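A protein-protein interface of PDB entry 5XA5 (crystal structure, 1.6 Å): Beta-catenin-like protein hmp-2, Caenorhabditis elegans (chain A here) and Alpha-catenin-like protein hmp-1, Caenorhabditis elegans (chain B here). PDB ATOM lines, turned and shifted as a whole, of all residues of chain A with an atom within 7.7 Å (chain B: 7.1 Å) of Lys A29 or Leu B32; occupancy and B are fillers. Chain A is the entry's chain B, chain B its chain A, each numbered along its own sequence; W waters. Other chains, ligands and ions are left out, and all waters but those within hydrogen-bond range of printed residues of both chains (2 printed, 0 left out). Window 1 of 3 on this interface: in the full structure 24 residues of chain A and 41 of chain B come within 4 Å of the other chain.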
ATOM      1  N   MET A  23      21.831 -11.356  14.102  1.00  0.00           N
ATOM      2  CA  MET A  23      22.752 -10.591  14.952  1.00  0.00           C
ATOM      3  C   MET A  23      22.787 -11.114  16.403  1.00  0.00           C
ATOM      4  O   MET A  23      23.864 -11.292  16.949  1.00  0.00           O
ATOM      5  CB  MET A  23      22.411  -9.085  14.911  1.00  0.00           C
ATOM      6  CG  MET A  23      23.413  -8.172  15.623  1.00  0.00           C
ATOM      7  SD  MET A  23      23.122  -6.419  15.297  1.00  0.00           S
ATOM      8  CE  MET A  23      24.402  -5.608  16.249  1.00  0.00           C
ATOM      9  N   PRO A  24      21.626 -11.379  17.033  1.00  0.00           N
ATOM     10  CA  PRO A  24      21.715 -11.913  18.402  1.00  0.00           C
ATOM     11  C   PRO A  24      22.378 -13.290  18.511  1.00  0.00           C
ATOM     12  O   PRO A  24      22.997 -13.588  19.532  1.00  0.00           O
ATOM     13  CB  PRO A  24      20.251 -11.996  18.848  1.00  0.00           C
ATOM     14  CG  PRO A  24      19.448 -11.810  17.620  1.00  0.00           C
ATOM     15  CD  PRO A  24      20.251 -10.970  16.706  1.00  0.00           C
ATOM     16  N   THR A  25      22.235 -14.121  17.484  1.00  0.00           N
ATOM     17  CA  THR A  25      22.921 -15.408  17.440  1.00  0.00           C
ATOM     18  C   THR A  25      24.428 -15.197  17.430  1.00  0.00           C
ATOM     19  O   THR A  25      25.170 -15.862  18.161  1.00  0.00           O
ATOM     20  CB  THR A  25      22.509 -16.227  16.197  1.00  0.00           C
ATOM     21  OG1 THR A  25      21.114 -16.551  16.287  1.00  0.00           O
ATOM     22  CG2 THR A  25      23.330 -17.503  16.085  1.00  0.00           C
ATOM     23  N   GLN A  26      24.883 -14.279  16.585  1.00  0.00           N
ATOM     24  CA  GLN A  26      26.309 -13.992  16.499  1.00  0.00           C
ATOM     25  C   GLN A  26      26.841 -13.498  17.830  1.00  0.00           C
ATOM     26  O   GLN A  26      27.903 -13.908  18.272  1.00  0.00           O
ATOM     27  CB  GLN A  26      26.607 -12.959  15.415  1.00  0.00           C
ATOM     28  CG  GLN A  26      26.540 -13.518  14.006  1.00  0.00           C
ATOM     29  CD  GLN A  26      27.580 -14.603  13.747  1.00  0.00           C
ATOM     30  OE1 GLN A  26      28.739 -14.495  14.165  1.00  0.00           O
ATOM     31  NE2 GLN A  26      27.161 -15.665  13.067  1.00  0.00           N
ATOM     32  N   GLN A  27      26.090 -12.645  18.502  1.00  0.00           N
ATOM     33  CA  GLN A  27      26.631 -12.051  19.713  1.00  0.00           C
ATOM     34  C   GLN A  27      26.656 -13.075  20.820  1.00  0.00           C
ATOM     35  O   GLN A  27      27.586 -13.095  21.622  1.00  0.00           O
ATOM     36  CB  GLN A  27      25.793 -10.848  20.094  1.00  0.00           C
ATOM     37  CG  GLN A  27      25.575  -9.906  18.887  1.00  0.00           C
ATOM     38  CD  GLN A  27      24.609  -8.810  19.165  1.00  0.00           C
ATOM     39  OE1 GLN A  27      23.714  -8.954  19.998  1.00  0.00           O
ATOM     40  NE2 GLN A  27      24.775  -7.704  18.485  1.00  0.00           N
ATOM     41  N   LEU A  28      25.638 -13.926  20.864  1.00  0.00           N
ATOM     42  CA  LEU A  28      25.602 -15.002  21.849  1.00  0.00           C
ATOM     43  C   LEU A  28      26.742 -15.987  21.577  1.00  0.00           C
ATOM     44  O   LEU A  28      27.457 -16.373  22.490  1.00  0.00           O
ATOM     45  CB  LEU A  28      24.241 -15.711  21.840  1.00  0.00           C
ATOM     46  CG  LEU A  28      24.039 -16.811  22.895  1.00  0.00           C
ATOM     47  CD1 LEU A  28      24.393 -16.338  24.294  1.00  0.00           C
ATOM     48  CD2 LEU A  28      22.592 -17.305  22.837  1.00  0.00           C
ATOM     49  N   LYS A  29      26.914 -16.383  20.317  1.00  0.00           N
ATOM     50  CA  LYS A  29      28.044 -17.226  19.941  1.00  0.00           C
ATOM     51  C   LYS A  29      29.353 -16.605  20.414  1.00  0.00           C
ATOM     52  O   LYS A  29      30.184 -17.266  21.046  1.00  0.00           O
ATOM     53  CB  LYS A  29      28.081 -17.435  18.416  1.00  0.00           C
ATOM     54  CG  LYS A  29      29.186 -18.404  17.960  1.00  0.00           C
ATOM     55  CD  LYS A  29      29.413 -18.466  16.436  1.00  0.00           C
ATOM     56  CE  LYS A  29      29.897 -17.137  15.860  1.00  0.00           C
ATOM     57  NZ  LYS A  29      30.550 -17.309  14.538  1.00  0.00           N
ATOM     58  N   GLN A  30      29.527 -15.324  20.108  1.00  0.00           N
ATOM     59  CA  GLN A  30      30.759 -14.619  20.445  1.00  0.00           C
ATOM     60  C   GLN A  30      31.018 -14.651  21.949  1.00  0.00           C
ATOM     61  O   GLN A  30      32.149 -14.887  22.382  1.00  0.00           O
ATOM     62  CB  GLN A  30      30.698 -13.169  19.956  1.00  0.00           C
ATOM     63  CG  GLN A  30      32.001 -12.400  20.108  1.00  0.00           C
ATOM     64  CD  GLN A  30      33.005 -12.734  19.022  1.00  0.00           C
ATOM     65  OE1 GLN A  30      32.638 -12.935  17.863  1.00  0.00           O
ATOM     66  NE2 GLN A  30      34.281 -12.792  19.391  1.00  0.00           N
ATOM     67  N   SER A  31      29.973 -14.418  22.737  1.00  0.00           N
ATOM     68  CA  SER A  31      30.147 -14.316  24.188  1.00  0.00           C
ATOM     69  C   SER A  31      30.471 -15.672  24.813  1.00  0.00           C
ATOM     70  O   SER A  31      31.213 -15.731  25.800  1.00  0.00           O
ATOM     71  CB  SER A  31      28.901 -13.706  24.841  1.00  0.00           C
ATOM     72  OG  SER A  31      27.827 -14.631  24.879  1.00  0.00           O
ATOM     73  N   VAL A  32      29.942 -16.753  24.235  1.00  0.00           N
ATOM     74  CA  VAL A  32      30.261 -18.102  24.714  1.00  0.00           C
ATOM     75  C   VAL A  32      31.703 -18.460  24.371  1.00  0.00           C
ATOM     76  O   VAL A  32      32.449 -18.930  25.225  1.00  0.00           O
ATOM     77  CB  VAL A  32      29.304 -19.163  24.121  1.00  0.00           C
ATOM     78  CG1 VAL A  32      29.819 -20.572  24.363  1.00  0.00           C
ATOM     79  CG2 VAL A  32      27.893 -18.998  24.671  1.00  0.00           C
ATOM     80  N   MET A  33      32.101 -18.228  23.125  1.00  0.00           N
ATOM     81  CA  MET A  33      33.460 -18.569  22.713  1.00  0.00           C
ATOM     82  C   MET A  33      34.513 -17.749  23.477  1.00  0.00           C
ATOM     83  O   MET A  33      35.562 -18.274  23.848  1.00  0.00           O
ATOM     84  CB  MET A  33      33.620 -18.394  21.203  1.00  0.00           C
ATOM     85  CG  MET A  33      32.774 -19.377  20.381  1.00  0.00           C
ATOM     86  SD  MET A  33      33.167 -21.101  20.742  1.00  0.00           S
ATOM     87  CE  MET A  33      34.889 -21.168  20.233  1.00  0.00           C
ATOM     88  N   ASP A  34      34.223 -16.474  23.730  1.00  0.00           N
ATOM     89  CA  ASP A  34      35.134 -15.613  24.477  1.00  0.00           C
ATOM     90  C   ASP A  34      35.385 -16.157  25.876  1.00  0.00           C
ATOM     91  O   ASP A  34      36.506 -16.094  26.391  1.00  0.00           O
ATOM     92  CB  ASP A  34      34.581 -14.187  24.591  1.00  0.00           C
ATOM     93  CG  ASP A  34      34.731 -13.389  23.314  1.00  0.00           C
ATOM     94  OD1 ASP A  34      35.421 -13.861  22.386  1.00  0.00           O
ATOM     95  OD2 ASP A  34      34.162 -12.279  23.250  1.00  0.00           O
ATOM     96  N   LEU A  35      34.333 -16.675  26.500  1.00  0.00           N
ATOM     97  CA  LEU A  35      34.485 -17.218  27.848  1.00  0.00           C
ATOM     98  C   LEU A  35      35.231 -18.543  27.800  1.00  0.00           C
ATOM     99  O   LEU A  35      36.093 -18.798  28.632  1.00  0.00           O
ATOM    100  CB  LEU A  35      33.125 -17.399  28.531  1.00  0.00           C
ATOM    101  CG  LEU A  35      33.121 -17.820  30.011  1.00  0.00           C
ATOM    102  CD1 LEU A  35      31.977 -17.162  30.757  1.00  0.00           C
ATOM    103  CD2 LEU A  35      33.019 -19.328  30.139  1.00  0.00           C
ATOM    104  N   VAL B  25      20.533 -20.562   7.593  1.00  0.00           N
ATOM    105  CA  VAL B  25      20.536 -21.351   8.828  1.00  0.00           C
ATOM    106  C   VAL B  25      21.719 -22.313   8.860  1.00  0.00           C
ATOM    107  O   VAL B  25      22.387 -22.462   9.883  1.00  0.00           O
ATOM    108  CB  VAL B  25      19.231 -22.153   8.977  1.00  0.00           C
ATOM    109  CG1 VAL B  25      19.302 -23.088  10.176  1.00  0.00           C
ATOM    110  CG2 VAL B  25      18.061 -21.210   9.115  1.00  0.00           C
ATOM    111  N   LEU B  26      21.986 -22.962   7.731  1.00  0.00           N
ATOM    112  CA  LEU B  26      23.038 -23.972   7.679  1.00  0.00           C
ATOM    113  C   LEU B  26      24.379 -23.359   8.071  1.00  0.00           C
ATOM    114  O   LEU B  26      25.109 -23.928   8.882  1.00  0.00           O
ATOM    115  CB  LEU B  26      23.132 -24.602   6.277  1.00  0.00           C
ATOM    116  CG  LEU B  26      24.173 -25.725   6.137  1.00  0.00           C
ATOM    117  CD1 LEU B  26      23.938 -26.812   7.191  1.00  0.00           C
ATOM    118  CD2 LEU B  26      24.161 -26.326   4.743  1.00  0.00           C
ATOM    119  N   LYS B  27      24.693 -22.187   7.524  1.00  0.00           N
ATOM    120  CA  LYS B  27      25.997 -21.572   7.824  1.00  0.00           C
ATOM    121  C   LYS B  27      26.074 -21.162   9.281  1.00  0.00           C
ATOM    122  O   LYS B  27      27.103 -21.366   9.930  1.00  0.00           O
ATOM    123  CB  LYS B  27      26.248 -20.357   6.934  1.00  0.00           C
ATOM    124  CG  LYS B  27      26.501 -20.762   5.479  1.00  0.00           C
ATOM    125  CD  LYS B  27      27.156 -19.658   4.676  1.00  0.00           C
ATOM    126  CE  LYS B  27      26.328 -18.397   4.685  1.00  0.00           C
ATOM    127  NZ  LYS B  27      24.967 -18.646   4.129  1.00  0.00           N
ATOM    128  N   GLN B  28      24.978 -20.609   9.797  1.00  0.00           N
ATOM    129  CA  GLN B  28      24.961 -20.192  11.202  1.00  0.00           C
ATOM    130  C   GLN B  28      25.155 -21.375  12.137  1.00  0.00           C
ATOM    131  O   GLN B  28      25.937 -21.301  13.080  1.00  0.00           O
ATOM    132  CB  GLN B  28      23.641 -19.486  11.538  1.00  0.00           C
ATOM    133  CG  GLN B  28      23.528 -18.080  10.983  1.00  0.00           C
ATOM    134  CD  GLN B  28      22.219 -17.415  11.372  1.00  0.00           C
ATOM    135  OE1 GLN B  28      22.087 -16.863  12.465  1.00  0.00           O
ATOM    136  NE2 GLN B  28      21.237 -17.470  10.475  1.00  0.00           N
ATOM    137  N   ILE B  29      24.428 -22.463  11.908  1.00  0.00           N
ATOM    138  CA  ILE B  29      24.537 -23.603  12.811  1.00  0.00           C
ATOM    139  C   ILE B  29      25.890 -24.293  12.631  1.00  0.00           C
ATOM    140  O   ILE B  29      26.434 -24.828  13.586  1.00  0.00           O
ATOM    141  CB  ILE B  29      23.370 -24.632  12.638  1.00  0.00           C
ATOM    142  CG1 ILE B  29      23.407 -25.334  11.281  1.00  0.00           C
ATOM    143  CG2 ILE B  29      22.010 -23.967  12.866  1.00  0.00           C
ATOM    144  CD1 ILE B  29      22.298 -26.355  11.105  1.00  0.00           C
ATOM    145  N   THR B  30      26.456 -24.240  11.428  1.00  0.00           N
ATOM    146  CA  THR B  30      27.777 -24.838  11.235  1.00  0.00           C
ATOM    147  C   THR B  30      28.802 -24.080  12.072  1.00  0.00           C
ATOM    148  O   THR B  30      29.684 -24.687  12.695  1.00  0.00           O
ATOM    149  CB  THR B  30      28.150 -24.839   9.751  1.00  0.00           C
ATOM    150  OG1 THR B  30      27.179 -25.622   9.048  1.00  0.00           O
ATOM    151  CG2 THR B  30      29.511 -25.443   9.525  1.00  0.00           C
ATOM    152  N   GLN B  31      28.671 -22.759  12.114  1.00  0.00           N
ATOM    153  CA  GLN B  31      29.545 -21.943  12.966  1.00  0.00           C
ATOM    154  C   GLN B  31      29.364 -22.307  14.426  1.00  0.00           C
ATOM    155  O   GLN B  31      30.332 -22.520  15.153  1.00  0.00           O
ATOM    156  CB  GLN B  31      29.254 -20.455  12.794  1.00  0.00           C
ATOM    157  CG  GLN B  31      29.642 -19.853  11.465  1.00  0.00           C
ATOM    158  CD  GLN B  31      29.046 -18.473  11.279  1.00  0.00           C
ATOM    159  OE1 GLN B  31      29.020 -17.670  12.213  1.00  0.00           O
ATOM    160  NE2 GLN B  31      28.577 -18.180  10.069  1.00  0.00           N
ATOM    161  N   LEU B  32      28.108 -22.358  14.849  1.00  0.00           N
ATOM    162  CA  LEU B  32      27.795 -22.621  16.255  1.00  0.00           C
ATOM    163  C   LEU B  32      28.446 -23.921  16.718  1.00  0.00           C
ATOM    164  O   LEU B  32      29.207 -23.937  17.694  1.00  0.00           O
ATOM    165  CB  LEU B  32      26.279 -22.668  16.465  1.00  0.00           C
ATOM    166  CG  LEU B  32      25.580 -21.321  16.257  1.00  0.00           C
ATOM    167  CD1 LEU B  32      24.066 -21.491  16.098  1.00  0.00           C
ATOM    168  CD2 LEU B  32      25.913 -20.347  17.423  1.00  0.00           C
ATOM    169  N   ILE B  33      28.182 -24.996  15.987  1.00  0.00           N
ATOM    170  CA  ILE B  33      28.603 -26.332  16.383  1.00  0.00           C
ATOM    171  C   ILE B  33      30.096 -26.545  16.230  1.00  0.00           C
ATOM    172  O   ILE B  33      30.758 -27.045  17.141  1.00  0.00           O
ATOM    173  CB  ILE B  33      27.850 -27.398  15.577  1.00  0.00           C
ATOM    174  CG1 ILE B  33      26.352 -27.328  15.887  1.00  0.00           C
ATOM    175  CG2 ILE B  33      28.398 -28.788  15.878  1.00  0.00           C
ATOM    176  CD1 ILE B  33      26.037 -27.170  17.361  1.00  0.00           C
ATOM    177  N   ASN B  34      30.648 -26.164  15.083  1.00  0.00           N
ATOM    178  CA  ASN B  34      32.078 -26.364  14.871  1.00  0.00           C
ATOM    179  C   ASN B  34      32.959 -25.595  15.843  1.00  0.00           C
ATOM    180  O   ASN B  34      33.948 -26.133  16.350  1.00  0.00           O
ATOM    181  CB  ASN B  34      32.458 -25.965  13.445  1.00  0.00           C
ATOM    182  CG  ASN B  34      32.018 -26.985  12.423  1.00  0.00           C
ATOM    183  OD1 ASN B  34      31.467 -28.037  12.764  1.00  0.00           O
ATOM    184  ND2 ASN B  34      32.287 -26.695  11.159  1.00  0.00           N
ATOM    185  N   GLU B  35      32.623 -24.336  16.103  1.00  0.00           N
ATOM    186  CA  GLU B  35      33.519 -23.519  16.918  1.00  0.00           C
ATOM    187  C   GLU B  35      33.582 -24.040  18.343  1.00  0.00           C
ATOM    188  O   GLU B  35      34.665 -24.141  18.909  1.00  0.00           O
ATOM    189  CB  GLU B  35      33.095 -22.052  16.922  1.00  0.00           C
ATOM    190  CG  GLU B  35      33.394 -21.316  15.620  1.00  0.00           C
ATOM    191  CD  GLU B  35      32.905 -19.883  15.640  1.00  0.00           C
ATOM    192  OE1 GLU B  35      33.038 -19.234  16.692  1.00  0.00           O
ATOM    193  OE2 GLU B  35      32.392 -19.405  14.603  1.00  0.00           O
ATOM    194  N   VAL B  36      32.436 -24.393  18.914  1.00  0.00           N
ATOM    195  CA  VAL B  36      32.401 -24.724  20.338  1.00  0.00           C
ATOM    196  C   VAL B  36      32.912 -26.141  20.601  1.00  0.00           C
ATOM    197  O   VAL B  36      33.300 -26.469  21.722  1.00  0.00           O
ATOM    198  CB  VAL B  36      30.978 -24.550  20.915  1.00  0.00           C
ATOM    199  CG1 VAL B  36      30.057 -25.670  20.455  1.00  0.00           C
ATOM    200  CG2 VAL B  36      31.025 -24.458  22.454  1.00  0.00           C
ATOM    201  N   THR B  37      32.937 -26.979  19.568  1.00  0.00           N
ATOM    202  CA  THR B  37      33.442 -28.341  19.723  1.00  0.00           C
ATOM    203  C   THR B  37      34.878 -28.504  19.223  1.00  0.00           C
ATOM    204  O   THR B  37      35.409 -29.615  19.210  1.00  0.00           O
ATOM    205  CB  THR B  37      32.557 -29.368  18.979  1.00  0.00           C
ATOM    206  OG1 THR B  37      32.626 -29.133  17.571  1.00  0.00           O
ATOM    207  CG2 THR B  37      31.113 -29.284  19.441  1.00  0.00           C
ATOM    208  N   ALA B  61      24.028 -11.323  26.613  1.00  0.00           N
ATOM    209  CA  ALA B  61      23.825 -11.877  25.273  1.00  0.00           C
ATOM    210  C   ALA B  61      22.703 -12.906  25.281  1.00  0.00           C
ATOM    211  O   ALA B  61      21.914 -12.967  24.334  1.00  0.00           O
ATOM    212  CB  ALA B  61      25.110 -12.497  24.731  1.00  0.00           C
ATOM    213  N   PHE B  65      19.129 -12.311  23.252  1.00  0.00           N
ATOM    214  CA  PHE B  65      18.626 -13.358  22.370  1.00  0.00           C
ATOM    215  C   PHE B  65      17.168 -13.668  22.729  1.00  0.00           C
ATOM    216  O   PHE B  65      16.304 -13.797  21.853  1.00  0.00           O
ATOM    217  CB  PHE B  65      19.499 -14.621  22.469  1.00  0.00           C
ATOM    218  CG  PHE B  65      19.174 -15.671  21.438  1.00  0.00           C
ATOM    219  CD1 PHE B  65      19.887 -15.740  20.253  1.00  0.00           C
ATOM    220  CD2 PHE B  65      18.157 -16.586  21.657  1.00  0.00           C
ATOM    221  CE1 PHE B  65      19.590 -16.703  19.298  1.00  0.00           C
ATOM    222  CE2 PHE B  65      17.838 -17.544  20.699  1.00  0.00           C
ATOM    223  CZ  PHE B  65      18.558 -17.606  19.521  1.00  0.00           C
ATOM    224  N   GLY B 127      28.472 -25.079  27.078  1.00  0.00           N
ATOM    225  CA  GLY B 127      28.492 -24.251  25.879  1.00  0.00           C
ATOM    226  C   GLY B 127      27.974 -25.006  24.677  1.00  0.00           C
ATOM    227  O   GLY B 127      27.208 -24.464  23.880  1.00  0.00           O
ATOM    228  N   ARG B 128      28.395 -26.260  24.541  1.00  0.00           N
ATOM    229  CA  ARG B 128      27.879 -27.119  23.475  1.00  0.00           C
ATOM    230  C   ARG B 128      26.363 -27.249  23.561  1.00  0.00           C
ATOM    231  O   ARG B 128      25.656 -27.118  22.567  1.00  0.00           O
ATOM    232  CB  ARG B 128      28.519 -28.503  23.531  1.00  0.00           C
ATOM    233  CG  ARG B 128      27.914 -29.496  22.552  1.00  0.00           C
ATOM    234  CD  ARG B 128      28.673 -30.806  22.577  1.00  0.00           C
ATOM    235  NE  ARG B 128      27.993 -31.854  21.824  1.00  0.00           N
ATOM    236  CZ  ARG B 128      28.554 -33.014  21.498  1.00  0.00           C
ATOM    237  NH1 ARG B 128      29.807 -33.262  21.854  1.00  0.00           N
ATOM    238  NH2 ARG B 128      27.870 -33.919  20.811  1.00  0.00           N
ATOM    239  N   LEU B 130      24.208 -25.229  25.022  1.00  0.00           N
ATOM    240  CA  LEU B 130      23.544 -23.945  24.781  1.00  0.00           C
ATOM    241  C   LEU B 130      23.508 -23.601  23.300  1.00  0.00           C
ATOM    242  O   LEU B 130      22.466 -23.214  22.775  1.00  0.00           O
ATOM    243  CB  LEU B 130      24.230 -22.804  25.545  1.00  0.00           C
ATOM    244  CG  LEU B 130      23.814 -21.368  25.169  1.00  0.00           C
ATOM    245  CD1 LEU B 130      22.312 -21.120  25.355  1.00  0.00           C
ATOM    246  CD2 LEU B 130      24.629 -20.339  25.951  1.00  0.00           C
ATOM    247  N   LEU B 131      24.645 -23.731  22.628  1.00  0.00           N
ATOM    248  CA  LEU B 131      24.702 -23.349  21.216  1.00  0.00           C
ATOM    249  C   LEU B 131      23.946 -24.357  20.345  1.00  0.00           C
ATOM    250  O   LEU B 131      23.466 -24.019  19.258  1.00  0.00           O
ATOM    251  CB  LEU B 131      26.163 -23.201  20.753  1.00  0.00           C
ATOM    252  CG  LEU B 131      26.945 -22.079  21.459  1.00  0.00           C
ATOM    253  CD1 LEU B 131      28.299 -21.878  20.806  1.00  0.00           C
ATOM    254  CD2 LEU B 131      26.164 -20.765  21.462  1.00  0.00           C
ATOM    255  N   THR B 132      23.812 -25.587  20.833  1.00  0.00           N
ATOM    256  CA  THR B 132      22.988 -26.589  20.156  1.00  0.00           C
ATOM    257  C   THR B 132      21.508 -26.225  20.279  1.00  0.00           C
ATOM    258  O   THR B 132      20.712 -26.425  19.346  1.00  0.00           O
ATOM    259  CB  THR B 132      23.238 -27.989  20.737  1.00  0.00           C
ATOM    260  OG1 THR B 132      24.552 -28.423  20.370  1.00  0.00           O
ATOM    261  CG2 THR B 132      22.221 -28.985  20.200  1.00  0.00           C
ATOM    262  N   ALA B 133      21.127 -25.696  21.442  1.00  0.00           N
ATOM    263  CA  ALA B 133      19.746 -25.260  21.653  1.00  0.00           C
ATOM    264  C   ALA B 133      19.443 -24.035  20.795  1.00  0.00           C
ATOM    265  O   ALA B 133      18.324 -23.867  20.305  1.00  0.00           O
ATOM    266  CB  ALA B 133      19.490 -24.966  23.122  1.00  0.00           C
ATOM    267  N   VAL B 134      20.446 -23.184  20.598  1.00  0.00           N
ATOM    268  CA  VAL B 134      20.297 -22.048  19.694  1.00  0.00           C
ATOM    269  C   VAL B 134      20.100 -22.550  18.269  1.00  0.00           C
ATOM    270  O   VAL B 134      19.224 -22.067  17.557  1.00  0.00           O
ATOM    271  CB  VAL B 134      21.520 -21.099  19.767  1.00  0.00           C
ATOM    272  CG1 VAL B 134      21.452 -20.053  18.669  1.00  0.00           C
ATOM    273  CG2 VAL B 134      21.568 -20.458  21.142  1.00  0.00           C
ATOM    274  N   ALA B 135      20.892 -23.544  17.878  1.00  0.00           N
ATOM    275  CA  ALA B 135      20.788 -24.112  16.533  1.00  0.00           C
ATOM    276  C   ALA B 135      19.416 -24.747  16.294  1.00  0.00           C
ATOM    277  O   ALA B 135      18.828 -24.568  15.222  1.00  0.00           O
ATOM    278  CB  ALA B 135      21.896 -25.134  16.303  1.00  0.00           C
ATOM    279  N   LYS B 136      18.903 -25.477  17.288  1.00  0.00           N
ATOM    280  CA  LYS B 136      17.586 -26.106  17.153  1.00  0.00           C
ATOM    281  C   LYS B 136      16.496 -25.047  17.029  1.00  0.00           C
ATOM    282  O   LYS B 136      15.530 -25.228  16.279  1.00  0.00           O
ATOM    283  CB  LYS B 136      17.302 -27.047  18.331  1.00  0.00           C
ATOM    284  CG  LYS B 136      17.958 -28.409  18.166  1.00  0.00           C
ATOM    285  CD  LYS B 136      17.827 -29.285  19.399  1.00  0.00           C
ATOM    286  CE  LYS B 136      18.552 -30.605  19.186  1.00  0.00           C
ATOM    287  NZ  LYS B 136      18.492 -31.486  20.383  1.00  0.00           N
ATOM    288  N   LEU B 138      16.858 -22.085  15.629  1.00  0.00           N
ATOM    289  CA  LEU B 138      16.930 -21.524  14.292  1.00  0.00           C
ATOM    290  C   LEU B 138      16.309 -22.463  13.273  1.00  0.00           C
ATOM    291  O   LEU B 138      15.707 -22.001  12.310  1.00  0.00           O
ATOM    292  CB  LEU B 138      18.374 -21.213  13.893  1.00  0.00           C
ATOM    293  CG  LEU B 138      19.070 -20.156  14.754  1.00  0.00           C
ATOM    294  CD1 LEU B 138      20.492 -19.980  14.290  1.00  0.00           C
ATOM    295  CD2 LEU B 138      18.319 -18.843  14.657  1.00  0.00           C
HETATM  296  O   HOH W   1      24.288 -15.561  13.087  1.00  0.00           O
HETATM  297  O   HOH W   2      22.659 -12.062  21.739  1.00  0.00           O
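NE2 of Gln A26 lies within hydrogen-bond range of OE1 of Gln B31, at 2.9 Å.
NZ of Lys A29 lies within hydrogen-bond range of OE1 of Gln B31 (2.8 Å).
OE2 of Glu B35 is in salt-bridge range of NZ of Lys A29, 2.8 Å away.
NZ of Lys A29 lies close to OE1 of Gln A26 (3.4 Å).
O of Leu A28 lies within hydrogen-bond range of OG of Ser A31 (3.0 Å).
O of Pro A24 touches CD1 of Phe B65, 3.9 Å away.
Thr A25 touches Gln B28 (CB to OE1, 3.8 Å).
Phe B65 touches Thr A25 (CE1 to OG1, 3.4 Å).
CA of Leu A28 touches CB of Ala B61 (3.9 Å).
CG2 of Val B134 touches CD2 of Leu A28, 3.7 Å away.
Lys A29 touches Leu B32.
Ala B61 touches Ser A31.
Val A32 touches Leu B130.
Met A33 touches Glu B35 (CE to O, 3.3 Å).
SD of Met A33 touches CA of Val B36, 3.7 Å away.
Lys A29 touches just these residues of chain B: Gln B31, Leu B32 and Glu B35.
Of the printed residues of chain B, Met A33 touches Glu B35 and Val B36.
Leu B32 touches just one residue of chain A: Lys A29.
Printed residues of chain A within 4 Å of Leu B138: Thr A25.
The nearest residue of chain B that does not touch Lys A29 is Leu B131 (4.3 Å).
The nearest printed residue of chain B that does not touch Leu A28 is Phe B65 (4.04 Å).
Along chain B the printed residues that touch a printed residue of chain A span positions 28 to 138.
Of the 13 printed residues of chain A, 8 touch a printed residue of chain B.
Hydrophobic or aromatic side chains of chain A within 4 Å of the printed part of chain B: Leu A28, Val A32 and Met A33.
Among the printed residues, Asp or Glu carboxylates within 4 Å of a Lys or Arg side-chain nitrogen of the other chain: Lys A29 with Glu B35 (2.8 Å).
Water W1 bridges OE1 of Gln B28 (2.6 Å) and NE2 of Gln A26 (2.9 Å).
Water W2 bridges the backbone carbonyl oxygen of Pro A24 (2.7 Å) and the backbone carbonyl oxygen of Ala B61 (2.8 Å).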
